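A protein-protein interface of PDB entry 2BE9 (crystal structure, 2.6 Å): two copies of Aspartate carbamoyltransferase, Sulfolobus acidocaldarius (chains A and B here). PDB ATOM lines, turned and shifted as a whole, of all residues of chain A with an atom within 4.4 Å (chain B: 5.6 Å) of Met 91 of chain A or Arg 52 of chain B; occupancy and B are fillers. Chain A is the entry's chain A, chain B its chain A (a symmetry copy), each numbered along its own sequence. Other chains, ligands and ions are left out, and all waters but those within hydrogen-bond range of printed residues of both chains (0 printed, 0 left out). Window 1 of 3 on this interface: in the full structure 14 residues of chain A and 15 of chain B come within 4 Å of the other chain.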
ATOM      1  N   GLU A  83      21.728  18.129  -4.562  1.00  0.00           N
ATOM      2  CA  GLU A  83      21.516  19.516  -4.200  1.00  0.00           C
ATOM      3  C   GLU A  83      21.999  19.839  -2.801  1.00  0.00           C
ATOM      4  O   GLU A  83      21.629  19.198  -1.832  1.00  0.00           O
ATOM      5  CB  GLU A  83      20.051  19.907  -4.356  1.00  0.00           C
ATOM      6  CG  GLU A  83      19.640  21.171  -3.603  1.00  0.00           C
ATOM      7  CD  GLU A  83      18.242  21.653  -3.985  1.00  0.00           C
ATOM      8  OE1 GLU A  83      18.112  22.303  -5.057  1.00  0.00           O
ATOM      9  OE2 GLU A  83      17.288  21.374  -3.205  1.00  0.00           O
ATOM     10  N   ASP A  87      21.064  25.772  -1.574  1.00  0.00           N
ATOM     11  CA  ASP A  87      20.046  25.834  -2.627  1.00  0.00           C
ATOM     12  C   ASP A  87      18.665  25.428  -2.135  1.00  0.00           C
ATOM     13  O   ASP A  87      17.649  26.025  -2.527  1.00  0.00           O
ATOM     14  CB  ASP A  87      20.455  25.004  -3.845  1.00  0.00           C
ATOM     15  CG  ASP A  87      21.504  25.697  -4.704  1.00  0.00           C
ATOM     16  OD1 ASP A  87      22.006  25.068  -5.655  1.00  0.00           O
ATOM     17  OD2 ASP A  87      21.833  26.883  -4.446  1.00  0.00           O
ATOM     18  N   THR A  88      18.618  24.426  -1.270  1.00  0.00           N
ATOM     19  CA  THR A  88      17.359  24.003  -0.704  1.00  0.00           C
ATOM     20  C   THR A  88      16.765  25.126   0.129  1.00  0.00           C
ATOM     21  O   THR A  88      15.569  25.414   0.021  1.00  0.00           O
ATOM     22  CB  THR A  88      17.518  22.715   0.125  1.00  0.00           C
ATOM     23  OG1 THR A  88      18.042  21.699  -0.725  1.00  0.00           O
ATOM     24  CG2 THR A  88      16.185  22.228   0.655  1.00  0.00           C
ATOM     25  N   ILE A  89      17.599  25.776   0.941  1.00  0.00           N
ATOM     26  CA  ILE A  89      17.105  26.859   1.778  1.00  0.00           C
ATOM     27  C   ILE A  89      16.584  28.024   0.925  1.00  0.00           C
ATOM     28  O   ILE A  89      15.523  28.596   1.237  1.00  0.00           O
ATOM     29  CB  ILE A  89      18.122  27.299   2.845  1.00  0.00           C
ATOM     30  CG1 ILE A  89      18.477  26.131   3.795  1.00  0.00           C
ATOM     31  CG2 ILE A  89      17.613  28.492   3.617  1.00  0.00           C
ATOM     32  CD1 ILE A  89      17.334  25.459   4.567  1.00  0.00           C
ATOM     33  N   ARG A  90      17.287  28.331  -0.171  1.00  0.00           N
ATOM     34  CA  ARG A  90      16.830  29.382  -1.096  1.00  0.00           C
ATOM     35  C   ARG A  90      15.461  29.052  -1.688  1.00  0.00           C
ATOM     36  O   ARG A  90      14.626  29.940  -1.844  1.00  0.00           O
ATOM     37  CB  ARG A  90      17.836  29.638  -2.217  1.00  0.00           C
ATOM     38  CG  ARG A  90      19.071  30.408  -1.795  1.00  0.00           C
ATOM     39  CD  ARG A  90      20.228  30.258  -2.784  1.00  0.00           C
ATOM     40  NE  ARG A  90      21.475  30.763  -2.208  1.00  0.00           N
ATOM     41  CZ  ARG A  90      22.639  30.110  -2.196  1.00  0.00           C
ATOM     42  NH1 ARG A  90      22.760  28.904  -2.754  1.00  0.00           N
ATOM     43  NH2 ARG A  90      23.695  30.661  -1.614  1.00  0.00           N
ATOM     44  N   MET A  91      15.240  27.774  -1.999  1.00  0.00           N
ATOM     45  CA  MET A  91      13.974  27.289  -2.543  1.00  0.00           C
ATOM     46  C   MET A  91      12.858  27.482  -1.511  1.00  0.00           C
ATOM     47  O   MET A  91      11.792  28.024  -1.841  1.00  0.00           O
ATOM     48  CB  MET A  91      14.118  25.829  -2.988  1.00  0.00           C
ATOM     49  CG  MET A  91      12.817  25.040  -3.227  1.00  0.00           C
ATOM     50  SD  MET A  91      12.997  23.208  -3.057  1.00  0.00           S
ATOM     51  CE  MET A  91      12.984  23.034  -1.269  1.00  0.00           C
ATOM     52  N   LEU A  92      13.102  27.099  -0.257  1.00  0.00           N
ATOM     53  CA  LEU A  92      12.048  27.255   0.755  1.00  0.00           C
ATOM     54  C   LEU A  92      11.647  28.693   1.000  1.00  0.00           C
ATOM     55  O   LEU A  92      10.482  28.976   1.284  1.00  0.00           O
ATOM     56  CB  LEU A  92      12.373  26.537   2.068  1.00  0.00           C
ATOM     57  CG  LEU A  92      12.502  25.022   1.870  1.00  0.00           C
ATOM     58  CD1 LEU A  92      13.172  24.372   3.057  1.00  0.00           C
ATOM     59  CD2 LEU A  92      11.141  24.426   1.553  1.00  0.00           C
ATOM     60  N   ASN A  93      12.606  29.597   0.851  1.00  0.00           N
ATOM     61  CA  ASN A  93      12.325  31.016   0.856  1.00  0.00           C
ATOM     62  C   ASN A  93      11.378  31.483  -0.247  1.00  0.00           C
ATOM     63  O   ASN A  93      10.616  32.389  -0.028  1.00  0.00           O
ATOM     64  CB  ASN A  93      13.621  31.825   0.833  1.00  0.00           C
ATOM     65  CG  ASN A  93      14.246  31.941   2.198  1.00  0.00           C
ATOM     66  OD1 ASN A  93      14.820  30.968   2.718  1.00  0.00           O
ATOM     67  ND2 ASN A  93      14.131  33.122   2.805  1.00  0.00           N
ATOM     68  N   ASN A  94      11.405  30.884  -1.431  1.00  0.00           N
ATOM     69  CA  ASN A  94      10.336  31.179  -2.393  1.00  0.00           C
ATOM     70  C   ASN A  94       9.017  30.755  -1.853  1.00  0.00           C
ATOM     71  O   ASN A  94       8.049  31.491  -1.965  1.00  0.00           O
ATOM     72  CB  ASN A  94      10.509  30.469  -3.728  1.00  0.00           C
ATOM     73  CG  ASN A  94      11.737  30.899  -4.436  1.00  0.00           C
ATOM     74  OD1 ASN A  94      12.133  32.070  -4.357  1.00  0.00           O
ATOM     75  ND2 ASN A  94      12.384  29.953  -5.130  1.00  0.00           N
ATOM     76  N   TYR A  95       8.970  29.576  -1.255  1.00  0.00           N
ATOM     77  CA  TYR A  95       7.678  28.941  -0.986  1.00  0.00           C
ATOM     78  C   TYR A  95       7.021  29.288   0.323  1.00  0.00           C
ATOM     79  O   TYR A  95       5.851  28.992   0.482  1.00  0.00           O
ATOM     80  CB  TYR A  95       7.790  27.423  -1.040  1.00  0.00           C
ATOM     81  CG  TYR A  95       8.381  26.863  -2.305  1.00  0.00           C
ATOM     82  CD1 TYR A  95       9.143  25.695  -2.261  1.00  0.00           C
ATOM     83  CD2 TYR A  95       8.167  27.481  -3.543  1.00  0.00           C
ATOM     84  CE1 TYR A  95       9.684  25.143  -3.415  1.00  0.00           C
ATOM     85  CE2 TYR A  95       8.708  26.946  -4.712  1.00  0.00           C
ATOM     86  CZ  TYR A  95       9.475  25.773  -4.635  1.00  0.00           C
ATOM     87  OH  TYR A  95      10.036  25.218  -5.758  1.00  0.00           O
ATOM     88  N   SER B  50       9.900  14.421  -6.916  1.00  0.00           N
ATOM     89  CA  SER B  50      10.675  15.668  -6.968  1.00  0.00           C
ATOM     90  C   SER B  50      10.078  16.639  -5.957  1.00  0.00           C
ATOM     91  O   SER B  50       8.950  17.117  -6.147  1.00  0.00           O
ATOM     92  CB  SER B  50      10.630  16.295  -8.354  1.00  0.00           C
ATOM     93  OG  SER B  50      10.677  17.719  -8.275  1.00  0.00           O
ATOM     94  N   THR B  51      10.827  16.953  -4.907  1.00  0.00           N
ATOM     95  CA  THR B  51      10.309  17.807  -3.848  1.00  0.00           C
ATOM     96  C   THR B  51      10.211  19.286  -4.276  1.00  0.00           C
ATOM     97  O   THR B  51       9.213  19.962  -3.951  1.00  0.00           O
ATOM     98  CB  THR B  51      11.060  17.607  -2.490  1.00  0.00           C
ATOM     99  OG1 THR B  51      10.823  16.277  -2.005  1.00  0.00           O
ATOM    100  CG2 THR B  51      10.577  18.587  -1.429  1.00  0.00           C
ATOM    101  N   ARG B  52      11.207  19.790  -5.016  1.00  0.00           N
ATOM    102  CA  ARG B  52      11.126  21.163  -5.508  1.00  0.00           C
ATOM    103  C   ARG B  52       9.811  21.415  -6.273  1.00  0.00           C
ATOM    104  O   ARG B  52       9.090  22.369  -5.971  1.00  0.00           O
ATOM    105  CB  ARG B  52      12.343  21.500  -6.376  1.00  0.00           C
ATOM    106  CG  ARG B  52      12.396  22.959  -6.882  1.00  0.00           C
ATOM    107  CD  ARG B  52      13.621  23.230  -7.807  1.00  0.00           C
ATOM    108  NE  ARG B  52      14.880  23.358  -7.062  1.00  0.00           N
ATOM    109  CZ  ARG B  52      15.314  24.486  -6.472  1.00  0.00           C
ATOM    110  NH1 ARG B  52      14.601  25.625  -6.515  1.00  0.00           N
ATOM    111  NH2 ARG B  52      16.483  24.483  -5.832  1.00  0.00           N
ATOM    112  N   THR B  53       9.492  20.558  -7.254  1.00  0.00           N
ATOM    113  CA  THR B  53       8.310  20.757  -8.125  1.00  0.00           C
ATOM    114  C   THR B  53       7.040  20.400  -7.384  1.00  0.00           C
ATOM    115  O   THR B  53       6.012  20.999  -7.597  1.00  0.00           O
ATOM    116  CB  THR B  53       8.437  19.965  -9.452  1.00  0.00           C
ATOM    117  OG1 THR B  53       9.795  20.043  -9.914  1.00  0.00           O
ATOM    118  CG2 THR B  53       7.533  20.526 -10.537  1.00  0.00           C
ATOM    119  N   TYR B  54       7.125  19.440  -6.480  1.00  0.00           N
ATOM    120  CA  TYR B  54       5.999  19.120  -5.628  1.00  0.00           C
ATOM    121  C   TYR B  54       5.519  20.390  -4.874  1.00  0.00           C
ATOM    122  O   TYR B  54       4.342  20.751  -4.910  1.00  0.00           O
ATOM    123  CB  TYR B  54       6.386  17.991  -4.653  1.00  0.00           C
ATOM    124  CG  TYR B  54       5.195  17.367  -3.976  1.00  0.00           C
ATOM    125  CD1 TYR B  54       4.484  18.048  -2.977  1.00  0.00           C
ATOM    126  CD2 TYR B  54       4.748  16.119  -4.353  1.00  0.00           C
ATOM    127  CE1 TYR B  54       3.334  17.470  -2.364  1.00  0.00           C
ATOM    128  CE2 TYR B  54       3.625  15.529  -3.752  1.00  0.00           C
ATOM    129  CZ  TYR B  54       2.915  16.205  -2.763  1.00  0.00           C
ATOM    130  OH  TYR B  54       1.805  15.602  -2.190  1.00  0.00           O
ATOM    131  N   LEU B  55       6.463  21.060  -4.222  1.00  0.00           N
ATOM    132  CA  LEU B  55       6.188  22.131  -3.296  1.00  0.00           C
ATOM    133  C   LEU B  55       5.729  23.368  -4.033  1.00  0.00           C
ATOM    134  O   LEU B  55       4.879  24.114  -3.553  1.00  0.00           O
ATOM    135  CB  LEU B  55       7.445  22.445  -2.504  1.00  0.00           C
ATOM    136  CG  LEU B  55       7.567  21.883  -1.093  1.00  0.00           C
ATOM    137  CD1 LEU B  55       6.864  20.559  -0.878  1.00  0.00           C
ATOM    138  CD2 LEU B  55       9.037  21.813  -0.728  1.00  0.00           C
ATOM    139  N   SER B  56       6.300  23.574  -5.203  1.00  0.00           N
ATOM    140  CA  SER B  56       5.924  24.653  -6.084  1.00  0.00           C
ATOM    141  C   SER B  56       4.434  24.577  -6.429  1.00  0.00           C
ATOM    142  O   SER B  56       3.686  25.550  -6.260  1.00  0.00           O
ATOM    143  CB  SER B  56       6.755  24.535  -7.355  1.00  0.00           C
ATOM    144  OG  SER B  56       6.292  25.469  -8.288  1.00  0.00           O
ATOM    145  N   PHE B  57       3.989  23.408  -6.885  1.00  0.00           N
ATOM    146  CA  PHE B  57       2.584  23.268  -7.224  1.00  0.00           C
ATOM    147  C   PHE B  57       1.683  23.375  -5.996  1.00  0.00           C
ATOM    148  O   PHE B  57       0.652  24.039  -6.022  1.00  0.00           O
ATOM    149  CB  PHE B  57       2.341  21.966  -7.947  1.00  0.00           C
ATOM    150  CG  PHE B  57       2.532  22.058  -9.430  1.00  0.00           C
ATOM    151  CD1 PHE B  57       3.664  21.497 -10.034  1.00  0.00           C
ATOM    152  CD2 PHE B  57       1.565  22.681 -10.233  1.00  0.00           C
ATOM    153  CE1 PHE B  57       3.832  21.556 -11.415  1.00  0.00           C
ATOM    154  CE2 PHE B  57       1.722  22.748 -11.604  1.00  0.00           C
ATOM    155  CZ  PHE B  57       2.862  22.187 -12.203  1.00  0.00           C
ATOM    156  N   LEU B 261      16.341  24.346 -11.688  1.00  0.00           N
ATOM    157  CA  LEU B 261      17.060  23.616 -10.645  1.00  0.00           C
ATOM    158  C   LEU B 261      16.584  22.133 -10.443  1.00  0.00           C
ATOM    159  O   LEU B 261      15.628  21.681 -11.076  1.00  0.00           O
ATOM    160  CB  LEU B 261      17.045  24.429  -9.348  1.00  0.00           C
ATOM    161  CG  LEU B 261      17.957  25.659  -9.185  1.00  0.00           C
ATOM    162  CD1 LEU B 261      19.234  25.575 -10.027  1.00  0.00           C
ATOM    163  CD2 LEU B 261      17.218  26.921  -9.447  1.00  0.00           C
ATOM    164  N   PRO B 262      17.268  21.348  -9.597  1.00  0.00           N
ATOM    165  CA  PRO B 262      18.490  21.611  -8.838  1.00  0.00           C
ATOM    166  C   PRO B 262      19.711  21.666  -9.749  1.00  0.00           C
ATOM    167  O   PRO B 262      19.668  21.169 -10.864  1.00  0.00           O
ATOM    168  CB  PRO B 262      18.576  20.399  -7.904  1.00  0.00           C
ATOM    169  CG  PRO B 262      17.870  19.289  -8.677  1.00  0.00           C
ATOM    170  CD  PRO B 262      16.749  19.980  -9.367  1.00  0.00           C
ATOM    171  N   ALA B 283      13.516  30.345 -10.571  1.00  0.00           N
ATOM    172  CA  ALA B 283      12.819  29.419  -9.665  1.00  0.00           C
ATOM    173  C   ALA B 283      11.720  30.149  -8.899  1.00  0.00           C
ATOM    174  O   ALA B 283      10.706  29.560  -8.583  1.00  0.00           O
ATOM    175  CB  ALA B 283      13.794  28.724  -8.720  1.00  0.00           C
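Among the printed residues, merely in contact across the chains: Glu 83 of chain A with Pro 262 of chain B, Met 91 of chain A with Arg 52 of chain B, Tyr 95 of chain A with Leu 55 of chain B, Tyr 95 of chain A with Ser 56 of chain B, Asp 87 of chain A with Arg 52 of chain B and Asn 94 of chain A with Ala 283 of chain B.
The side-chain carboxylate (OE1) of Glu 83 of chain A lies within salt-bridge range of the guanidinium group (NH2) of Arg 52 of chain B, 2.8 Å away.
The side-chain hydroxyl of Tyr 95 of chain A is in hydrogen-bond range of the backbone carbonyl oxygen of Arg 52 of chain B (3.0 Å).
The side-chain carboxylate (OD2) of Asp 87 of chain A lies within salt-bridge range of the guanidinium group (NH1) of Arg 90 of chain A.
OE2 of Glu 83 of chain A sits at hydrogen-bond distance from OG1 of Thr 88 of chain A, at 2.6 Å.
Printed residues of chain A within 4 Å of Arg 52 of chain B: Glu 83 (2.8 Å), Asp 87 (3.8 Å), Met 91 (3.6 Å) and Tyr 95 (3.0 Å).
Of the printed residues of chain B, Asn 94 of chain A touches Ala 283.
Printed residues of chain A within 4 Å of Ala 283 of chain B: Asn 94 (3.8 Å).
Of the printed residues of chain A, Pro 262 of chain B touches Glu 83.
Printed residues of chain A within 4 Å of Ser 56 of chain B: Tyr 95.
Leu 92 of chain A touches none of the printed residues of chain B.
The nearest residue of chain B that does not touch Met 91 of chain A is Leu 55 of chain B (4.2 Å).
Among the printed residues, 8 pairs touch across the chains.
Among the printed residues, Asp or Glu carboxylates within 4 Å of a Lys or Arg side-chain nitrogen of the other chain: Glu 83 of chain A with Arg 52 of chain B (2.8 Å).
No position is printed for both chains.
Of the 8 pairs that touch across the chains among the printed residues, none has its exchanged pair printed and touching as well.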
